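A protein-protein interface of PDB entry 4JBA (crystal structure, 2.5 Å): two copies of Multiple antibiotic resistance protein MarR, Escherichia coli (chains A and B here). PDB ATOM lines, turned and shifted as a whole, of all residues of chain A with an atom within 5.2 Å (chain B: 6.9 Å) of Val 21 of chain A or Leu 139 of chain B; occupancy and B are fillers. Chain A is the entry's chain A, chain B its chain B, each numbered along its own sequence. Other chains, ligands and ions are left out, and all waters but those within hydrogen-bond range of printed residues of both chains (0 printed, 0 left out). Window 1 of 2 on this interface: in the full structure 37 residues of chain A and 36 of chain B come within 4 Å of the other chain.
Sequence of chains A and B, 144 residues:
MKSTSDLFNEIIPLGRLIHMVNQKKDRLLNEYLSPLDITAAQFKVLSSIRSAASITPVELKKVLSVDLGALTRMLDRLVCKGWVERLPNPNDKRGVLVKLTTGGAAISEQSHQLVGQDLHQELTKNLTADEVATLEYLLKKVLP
Leu 135 of chain B touches Leu 14 of chain A. Glu 136 of chain B touches Leu 14 of chain A (OE2 to N, 3.99 Å). Leu 139 of chain B touches Leu 14 of chain A. Leu 17 of chain A touches Leu 139 of chain B. Leu 17 of chain A touches Lys 140 of chain B (CD2 to CG, 3.99 Å). Met 20 of chain A touches Leu 143 of chain B (CE to CD1, 3.998 Å). Val 21 of chain A touches Ile 18 of chain B. Asn 22 of chain A touches Ile 18 of chain B (ND2 to CG2, 3.6 Å). CD1 of Leu 135 of chain A touches CD1 of Leu 135 of chain B (3.4 Å). Leu 135 of chain A touches Leu 138 of chain B (N to CD1, 3.8 Å).
The side-chain amino group of Lys 24 of chain A lies within hydrogen-bond range of the backbone carbonyl oxygen of Val 142 of chain B, at 3.2 Å. The side-chain amino group of Lys 24 of chain A sits at hydrogen-bond distance from the backbone carbonyl oxygen of Leu 143 of chain B (3.1 Å). The side-chain amino group (NZ) of Lys 24 of chain A lies within salt-bridge range of the chain-end carboxylate (O) of Pro 144 of chain B (3.6 Å).
Of the printed residues of chain B, Val 21 of chain A touches Ile 18, Leu 139 and Leu 143. Printed residues of chain B within 4 Å of Asn 22 of chain A: Ile 18. Gln 23 of chain A touches none of the printed residues of chain B. Of the printed residues of chain B, Lys 24 of chain A touches Val 142, Leu 143 and Pro 144. Printed residues of chain A within 4 Å of Leu 14 of chain B: Leu 135 (3.9 Å) and Leu 139 (3.5 Å). Printed residues of chain A within 4 Å of Leu 135 of chain B: Leu 14 (3.7 Å) and Leu 135 (3.4 Å). Leu 139 of chain B touches three residues of chain A. Of the printed residues of chain A, Lys 140 of chain B touches Leu 17 (3.99 Å). Lys 141 of chain B touches none of the printed residues of chain A. The nearest residue of chain B that does not touch Val 21 of chain A is Val 142 of chain B (4.3 Å).
Leu 14 of chain A touches Leu 135 of chain B, and with the chains exchanged Leu 135 of chain A touches Leu 14 of chain B. Leu 14 of chain A touches Leu 139 of chain B, and with the chains exchanged Leu 139 of chain A touches Leu 14 of chain B. Leu 135 of chain B touches its own counterpart, Leu 135 of chain A. Positions printed for both chains: 14, 18, 135 and 139. Of the 18 pairs that touch across the chains among the printed residues, 5 have their exchanged pair printed and touching as well.
Of the 13 printed residues of chain B, 10 touch a printed residue of chain A. Along chain B the printed residues that touch a printed residue of chain A span positions 14 to 144. Printed residues of chain A that touch a printed residue of chain B: Leu 14, Leu 17, Met 20, Val 21, Asn 22, Lys 24, Leu 135 and Leu 139. Hydrophobic or aromatic side chains of chain A within 4 Å of the printed part of chain B: Leu 14, Leu 17, Met 20, Val 21, Leu 135 and Leu 139. Among the printed residues, no Asp or Glu carboxylate lies within 4 Å of a Lys or Arg side-chain nitrogen of the other chain.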
ATOM      1  N   LEU A  14     -19.163  19.681  17.139  1.00  0.00           N
ATOM      2  CA  LEU A  14     -17.800  20.038  16.819  1.00  0.00           C
ATOM      3  C   LEU A  14     -17.620  20.404  15.324  1.00  0.00           C
ATOM      4  O   LEU A  14     -16.910  21.362  14.987  1.00  0.00           O
ATOM      5  CB  LEU A  14     -16.879  18.890  17.205  1.00  0.00           C
ATOM      6  CG  LEU A  14     -15.390  19.172  17.243  1.00  0.00           C
ATOM      7  CD1 LEU A  14     -15.107  20.527  17.874  1.00  0.00           C
ATOM      8  CD2 LEU A  14     -14.701  18.063  18.013  1.00  0.00           C
ATOM      9  N   ARG A  16     -19.681  21.785  13.157  1.00  0.00           N
ATOM     10  CA  ARG A  16     -20.139  23.116  12.839  1.00  0.00           C
ATOM     11  C   ARG A  16     -19.228  24.152  13.448  1.00  0.00           C
ATOM     12  O   ARG A  16     -18.901  25.154  12.814  1.00  0.00           O
ATOM     13  CB  ARG A  16     -21.578  23.323  13.303  1.00  0.00           C
ATOM     14  CG  ARG A  16     -22.610  23.037  12.222  1.00  0.00           C
ATOM     15  CD  ARG A  16     -23.957  23.655  12.566  1.00  0.00           C
ATOM     16  NE  ARG A  16     -24.771  22.765  13.394  1.00  0.00           N
ATOM     17  CZ  ARG A  16     -25.535  23.170  14.409  1.00  0.00           C
ATOM     18  NH1 ARG A  16     -25.587  24.455  14.735  1.00  0.00           N
ATOM     19  NH2 ARG A  16     -26.243  22.287  15.102  1.00  0.00           N
ATOM     20  N   LEU A  17     -18.745  23.873  14.649  1.00  0.00           N
ATOM     21  CA  LEU A  17     -17.852  24.791  15.322  1.00  0.00           C
ATOM     22  C   LEU A  17     -16.579  25.000  14.538  1.00  0.00           C
ATOM     23  O   LEU A  17     -16.097  26.128  14.424  1.00  0.00           O
ATOM     24  CB  LEU A  17     -17.536  24.308  16.722  1.00  0.00           C
ATOM     25  CG  LEU A  17     -18.627  24.600  17.744  1.00  0.00           C
ATOM     26  CD1 LEU A  17     -18.275  23.996  19.097  1.00  0.00           C
ATOM     27  CD2 LEU A  17     -18.833  26.095  17.860  1.00  0.00           C
ATOM     28  N   ILE A  18     -16.031  23.917  13.987  1.00  0.00           N
ATOM     29  CA  ILE A  18     -14.863  24.028  13.106  1.00  0.00           C
ATOM     30  C   ILE A  18     -15.207  24.817  11.846  1.00  0.00           C
ATOM     31  O   ILE A  18     -14.494  25.737  11.468  1.00  0.00           O
ATOM     32  CB  ILE A  18     -14.312  22.651  12.710  1.00  0.00           C
ATOM     33  CG1 ILE A  18     -13.640  21.988  13.915  1.00  0.00           C
ATOM     34  CG2 ILE A  18     -13.327  22.785  11.555  1.00  0.00           C
ATOM     35  CD1 ILE A  18     -13.945  20.509  14.043  1.00  0.00           C
ATOM     36  N   HIS A  19     -16.321  24.470  11.225  1.00  0.00           N
ATOM     37  CA  HIS A  19     -16.815  25.217  10.099  1.00  0.00           C
ATOM     38  C   HIS A  19     -16.872  26.679  10.427  1.00  0.00           C
ATOM     39  O   HIS A  19     -16.226  27.499   9.772  1.00  0.00           O
ATOM     40  CB  HIS A  19     -18.183  24.702   9.684  1.00  0.00           C
ATOM     41  CG  HIS A  19     -18.855  25.539   8.636  1.00  0.00           C
ATOM     42  ND1 HIS A  19     -18.180  26.115   7.618  1.00  0.00           N
ATOM     43  CD2 HIS A  19     -20.203  25.868   8.446  1.00  0.00           C
ATOM     44  CE1 HIS A  19     -19.042  26.793   6.837  1.00  0.00           C
ATOM     45  NE2 HIS A  19     -20.275  26.637   7.341  1.00  0.00           N
ATOM     46  N   MET A  20     -17.551  27.007  11.516  1.00  0.00           N
ATOM     47  CA  MET A  20     -17.739  28.399  11.900  1.00  0.00           C
ATOM     48  C   MET A  20     -16.404  29.103  12.092  1.00  0.00           C
ATOM     49  O   MET A  20     -16.147  30.145  11.493  1.00  0.00           O
ATOM     50  CB  MET A  20     -18.585  28.494  13.172  1.00  0.00           C
ATOM     51  CG  MET A  20     -20.071  28.253  12.937  1.00  0.00           C
ATOM     52  SD  MET A  20     -21.016  27.892  14.441  1.00  0.00           S
ATOM     53  CE  MET A  20     -21.502  29.536  14.954  1.00  0.00           C
ATOM     54  N   VAL A  21     -15.535  28.493  12.882  1.00  0.00           N
ATOM     55  CA  VAL A  21     -14.251  29.088  13.215  1.00  0.00           C
ATOM     56  C   VAL A  21     -13.377  29.222  11.966  1.00  0.00           C
ATOM     57  O   VAL A  21     -12.626  30.186  11.820  1.00  0.00           O
ATOM     58  CB  VAL A  21     -13.529  28.261  14.297  1.00  0.00           C
ATOM     59  CG1 VAL A  21     -12.176  28.866  14.633  1.00  0.00           C
ATOM     60  CG2 VAL A  21     -14.393  28.166  15.538  1.00  0.00           C
ATOM     61  N   ASN A  22     -13.561  28.307  11.026  1.00  0.00           N
ATOM     62  CA  ASN A  22     -12.863  28.371   9.756  1.00  0.00           C
ATOM     63  C   ASN A  22     -13.309  29.550   8.904  1.00  0.00           C
ATOM     64  O   ASN A  22     -12.484  30.252   8.315  1.00  0.00           O
ATOM     65  CB  ASN A  22     -13.045  27.066   8.989  1.00  0.00           C
ATOM     66  CG  ASN A  22     -12.034  26.899   7.875  1.00  0.00           C
ATOM     67  OD1 ASN A  22     -12.369  26.489   6.800  1.00  0.00           O
ATOM     68  ND2 ASN A  22     -10.808  27.218   8.147  1.00  0.00           N
ATOM     69  N   GLN A  23     -14.618  29.771   8.843  1.00  0.00           N
ATOM     70  CA  GLN A  23     -15.153  30.914   8.120  1.00  0.00           C
ATOM     71  C   GLN A  23     -14.582  32.203   8.678  1.00  0.00           C
ATOM     72  O   GLN A  23     -14.216  33.103   7.926  1.00  0.00           O
ATOM     73  CB  GLN A  23     -16.685  30.937   8.183  1.00  0.00           C
ATOM     74  CG  GLN A  23     -17.367  29.859   7.341  1.00  0.00           C
ATOM     75  CD  GLN A  23     -17.370  30.180   5.841  1.00  0.00           C
ATOM     76  OE1 GLN A  23     -18.047  31.108   5.391  1.00  0.00           O
ATOM     77  NE2 GLN A  23     -16.646  29.378   5.060  1.00  0.00           N
ATOM     78  N   LYS A  24     -14.458  32.270  10.000  1.00  0.00           N
ATOM     79  CA  LYS A  24     -13.909  33.445  10.643  1.00  0.00           C
ATOM     80  C   LYS A  24     -12.453  33.634  10.272  1.00  0.00           C
ATOM     81  O   LYS A  24     -12.022  34.753   9.977  1.00  0.00           O
ATOM     82  CB  LYS A  24     -14.070  33.371  12.163  1.00  0.00           C
ATOM     83  CG  LYS A  24     -13.251  34.407  12.922  1.00  0.00           C
ATOM     84  CD  LYS A  24     -14.041  35.040  14.059  1.00  0.00           C
ATOM     85  CE  LYS A  24     -13.109  35.593  15.137  1.00  0.00           C
ATOM     86  NZ  LYS A  24     -13.773  36.626  15.988  1.00  0.00           N
ATOM     87  N   LYS A  25     -11.700  32.541  10.245  1.00  0.00           N
ATOM     88  CA  LYS A  25     -10.302  32.615   9.843  1.00  0.00           C
ATOM     89  C   LYS A  25     -10.159  33.222   8.455  1.00  0.00           C
ATOM     90  O   LYS A  25      -9.310  34.083   8.239  1.00  0.00           O
ATOM     91  CB  LYS A  25      -9.619  31.241   9.893  1.00  0.00           C
ATOM     92  CG  LYS A  25      -8.129  31.312   9.566  1.00  0.00           C
ATOM     93  CD  LYS A  25      -7.519  29.950   9.299  1.00  0.00           C
ATOM     94  CE  LYS A  25      -8.364  29.124   8.340  1.00  0.00           C
ATOM     95  NZ  LYS A  25      -7.971  29.339   6.926  1.00  0.00           N
ATOM     96  N   LEU A 135      -6.441  24.647  23.477  1.00  0.00           N
ATOM     97  CA  LEU A 135      -7.166  24.547  22.209  1.00  0.00           C
ATOM     98  C   LEU A 135      -6.274  23.937  21.110  1.00  0.00           C
ATOM     99  O   LEU A 135      -6.662  22.973  20.428  1.00  0.00           O
ATOM    100  CB  LEU A 135      -7.648  25.916  21.795  1.00  0.00           C
ATOM    101  CG  LEU A 135      -8.263  26.071  20.412  1.00  0.00           C
ATOM    102  CD1 LEU A 135      -9.430  25.097  20.235  1.00  0.00           C
ATOM    103  CD2 LEU A 135      -8.724  27.513  20.256  1.00  0.00           C
ATOM    104  N   LEU A 139      -7.025  20.432  19.365  1.00  0.00           N
ATOM    105  CA  LEU A 139      -7.212  20.407  17.925  1.00  0.00           C
ATOM    106  C   LEU A 139      -6.307  19.328  17.319  1.00  0.00           C
ATOM    107  O   LEU A 139      -6.791  18.396  16.643  1.00  0.00           O
ATOM    108  CB  LEU A 139      -6.934  21.769  17.320  1.00  0.00           C
ATOM    109  CG  LEU A 139      -8.106  22.770  17.429  1.00  0.00           C
ATOM    110  CD1 LEU A 139      -7.667  24.172  17.021  1.00  0.00           C
ATOM    111  CD2 LEU A 139      -9.270  22.330  16.560  1.00  0.00           C
ATOM    112  N   LEU B  14      -2.474  28.451  15.300  1.00  0.00           N
ATOM    113  CA  LEU B  14      -3.868  28.079  15.438  1.00  0.00           C
ATOM    114  C   LEU B  14      -4.584  28.115  14.100  1.00  0.00           C
ATOM    115  O   LEU B  14      -5.471  27.287  13.823  1.00  0.00           O
ATOM    116  CB  LEU B  14      -4.549  29.022  16.415  1.00  0.00           C
ATOM    117  CG  LEU B  14      -5.986  28.729  16.817  1.00  0.00           C
ATOM    118  CD1 LEU B  14      -6.148  27.270  17.217  1.00  0.00           C
ATOM    119  CD2 LEU B  14      -6.373  29.646  17.962  1.00  0.00           C
ATOM    120  N   ILE B  18      -6.746  24.913  12.584  1.00  0.00           N
ATOM    121  CA  ILE B  18      -8.137  24.981  12.159  1.00  0.00           C
ATOM    122  C   ILE B  18      -8.282  24.583  10.695  1.00  0.00           C
ATOM    123  O   ILE B  18      -9.214  23.868  10.334  1.00  0.00           O
ATOM    124  CB  ILE B  18      -8.705  26.389  12.329  1.00  0.00           C
ATOM    125  CG1 ILE B  18      -8.842  26.733  13.808  1.00  0.00           C
ATOM    126  CG2 ILE B  18     -10.031  26.519  11.601  1.00  0.00           C
ATOM    127  CD1 ILE B  18      -8.494  28.172  14.121  1.00  0.00           C
ATOM    128  N   THR B 134     -14.283  20.769  26.589  1.00  0.00           N
ATOM    129  CA  THR B 134     -13.320  21.852  26.702  1.00  0.00           C
ATOM    130  C   THR B 134     -13.075  22.458  25.340  1.00  0.00           C
ATOM    131  O   THR B 134     -13.057  23.677  25.192  1.00  0.00           O
ATOM    132  CB  THR B 134     -11.978  21.350  27.273  1.00  0.00           C
ATOM    133  OG1 THR B 134     -12.165  20.916  28.627  1.00  0.00           O
ATOM    134  CG2 THR B 134     -10.946  22.438  27.248  1.00  0.00           C
ATOM    135  N   LEU B 135     -12.915  21.602  24.336  1.00  0.00           N
ATOM    136  CA  LEU B 135     -12.570  22.061  22.996  1.00  0.00           C
ATOM    137  C   LEU B 135     -13.722  22.875  22.413  1.00  0.00           C
ATOM    138  O   LEU B 135     -13.531  23.997  21.964  1.00  0.00           O
ATOM    139  CB  LEU B 135     -12.243  20.870  22.092  1.00  0.00           C
ATOM    140  CG  LEU B 135     -12.189  21.123  20.584  1.00  0.00           C
ATOM    141  CD1 LEU B 135     -11.068  22.084  20.236  1.00  0.00           C
ATOM    142  CD2 LEU B 135     -12.023  19.806  19.832  1.00  0.00           C
ATOM    143  N   GLU B 136     -14.933  22.336  22.510  1.00  0.00           N
ATOM    144  CA  GLU B 136     -16.130  23.075  22.120  1.00  0.00           C
ATOM    145  C   GLU B 136     -16.206  24.432  22.816  1.00  0.00           C
ATOM    146  O   GLU B 136     -16.328  25.461  22.163  1.00  0.00           O
ATOM    147  CB  GLU B 136     -17.383  22.250  22.391  1.00  0.00           C
ATOM    148  CG  GLU B 136     -17.498  21.005  21.506  1.00  0.00           C
ATOM    149  CD  GLU B 136     -18.706  20.132  21.844  1.00  0.00           C
ATOM    150  OE1 GLU B 136     -19.387  20.400  22.864  1.00  0.00           O
ATOM    151  OE2 GLU B 136     -18.974  19.165  21.091  1.00  0.00           O
ATOM    152  N   TYR B 137     -16.013  24.436  24.126  1.00  0.00           N
ATOM    153  CA  TYR B 137     -16.053  25.678  24.897  1.00  0.00           C
ATOM    154  C   TYR B 137     -15.068  26.709  24.346  1.00  0.00           C
ATOM    155  O   TYR B 137     -15.390  27.883  24.240  1.00  0.00           O
ATOM    156  CB  TYR B 137     -15.764  25.399  26.380  1.00  0.00           C
ATOM    157  CG  TYR B 137     -15.673  26.650  27.236  1.00  0.00           C
ATOM    158  CD1 TYR B 137     -16.801  27.429  27.491  1.00  0.00           C
ATOM    159  CD2 TYR B 137     -14.466  27.036  27.807  1.00  0.00           C
ATOM    160  CE1 TYR B 137     -16.716  28.578  28.261  1.00  0.00           C
ATOM    161  CE2 TYR B 137     -14.378  28.160  28.603  1.00  0.00           C
ATOM    162  CZ  TYR B 137     -15.502  28.937  28.813  1.00  0.00           C
ATOM    163  OH  TYR B 137     -15.409  30.060  29.590  1.00  0.00           O
ATOM    164  N   LEU B 138     -13.858  26.263  24.012  1.00  0.00           N
ATOM    165  CA  LEU B 138     -12.788  27.179  23.699  1.00  0.00           C
ATOM    166  C   LEU B 138     -12.932  27.657  22.264  1.00  0.00           C
ATOM    167  O   LEU B 138     -12.584  28.806  21.934  1.00  0.00           O
ATOM    168  CB  LEU B 138     -11.433  26.508  23.901  1.00  0.00           C
ATOM    169  CG  LEU B 138     -11.039  26.154  25.349  1.00  0.00           C
ATOM    170  CD1 LEU B 138      -9.632  25.566  25.409  1.00  0.00           C
ATOM    171  CD2 LEU B 138     -11.149  27.372  26.255  1.00  0.00           C
ATOM    172  N   LEU B 139     -13.448  26.778  21.408  1.00  0.00           N
ATOM    173  CA  LEU B 139     -13.770  27.137  20.035  1.00  0.00           C
ATOM    174  C   LEU B 139     -14.791  28.281  19.977  1.00  0.00           C
ATOM    175  O   LEU B 139     -14.578  29.272  19.291  1.00  0.00           O
ATOM    176  CB  LEU B 139     -14.281  25.917  19.270  1.00  0.00           C
ATOM    177  CG  LEU B 139     -13.206  25.015  18.636  1.00  0.00           C
ATOM    178  CD1 LEU B 139     -13.837  23.784  18.008  1.00  0.00           C
ATOM    179  CD2 LEU B 139     -12.400  25.780  17.590  1.00  0.00           C
ATOM    180  N   LYS B 140     -15.842  28.182  20.780  1.00  0.00           N
ATOM    181  CA  LYS B 140     -16.797  29.269  20.911  1.00  0.00           C
ATOM    182  C   LYS B 140     -16.122  30.574  21.332  1.00  0.00           C
ATOM    183  O   LYS B 140     -16.530  31.643  20.913  1.00  0.00           O
ATOM    184  CB  LYS B 140     -17.904  28.907  21.908  1.00  0.00           C
ATOM    185  CG  LYS B 140     -18.739  27.695  21.515  1.00  0.00           C
ATOM    186  CD  LYS B 140     -19.821  27.414  22.550  1.00  0.00           C
ATOM    187  CE  LYS B 140     -20.582  26.135  22.235  1.00  0.00           C
ATOM    188  NZ  LYS B 140     -21.244  25.564  23.453  1.00  0.00           N
ATOM    189  N   LYS B 141     -15.139  30.483  22.221  1.00  0.00           N
ATOM    190  CA  LYS B 141     -14.530  31.689  22.792  1.00  0.00           C
ATOM    191  C   LYS B 141     -13.751  32.483  21.741  1.00  0.00           C
ATOM    192  O   LYS B 141     -13.475  33.670  21.923  1.00  0.00           O
ATOM    193  CB  LYS B 141     -13.629  31.340  23.978  1.00  0.00           C
ATOM    194  CG  LYS B 141     -14.251  31.631  25.332  1.00  0.00           C
ATOM    195  CD  LYS B 141     -13.300  31.301  26.473  1.00  0.00           C
ATOM    196  CE  LYS B 141     -13.404  32.330  27.580  1.00  0.00           C
ATOM    197  NZ  LYS B 141     -12.081  32.638  28.191  1.00  0.00           N
ATOM    198  N   VAL B 142     -13.413  31.827  20.636  1.00  0.00           N
ATOM    199  CA  VAL B 142     -12.725  32.493  19.537  1.00  0.00           C
ATOM    200  C   VAL B 142     -13.680  33.413  18.772  1.00  0.00           C
ATOM    201  O   VAL B 142     -13.274  34.470  18.278  1.00  0.00           O
ATOM    202  CB  VAL B 142     -12.107  31.478  18.555  1.00  0.00           C
ATOM    203  CG1 VAL B 142     -11.540  32.190  17.345  1.00  0.00           C
ATOM    204  CG2 VAL B 142     -11.023  30.660  19.243  1.00  0.00           C
ATOM    205  N   LEU B 143     -14.968  33.061  18.791  1.00  0.00           N
ATOM    206  CA  LEU B 143     -15.934  33.523  17.783  1.00  0.00           C
ATOM    207  C   LEU B 143     -16.390  34.976  17.963  1.00  0.00           C
ATOM    208  O   LEU B 143     -16.541  35.709  16.978  1.00  0.00           O
ATOM    209  CB  LEU B 143     -17.143  32.599  17.744  1.00  0.00           C
ATOM    210  CG  LEU B 143     -16.924  31.287  17.012  1.00  0.00           C
ATOM    211  CD1 LEU B 143     -18.195  30.467  16.999  1.00  0.00           C
ATOM    212  CD2 LEU B 143     -16.428  31.532  15.592  1.00  0.00           C
ATOM    213  N   PRO B 144     -16.672  35.380  19.216  1.00  0.00           N
ATOM    214  CA  PRO B 144     -16.754  36.808  19.519  1.00  0.00           C
ATOM    215  C   PRO B 144     -15.421  37.510  19.240  1.00  0.00           C
ATOM    216  O   PRO B 144     -14.345  36.965  19.507  1.00  0.00           O
ATOM    217  CB  PRO B 144     -17.059  36.827  21.020  1.00  0.00           C
ATOM    218  CG  PRO B 144     -17.757  35.540  21.276  1.00  0.00           C
ATOM    219  CD  PRO B 144     -17.135  34.545  20.342  1.00  0.00           C
ATOM    220  OXT PRO B 144     -15.388  38.626  18.717  1.00  0.00           O
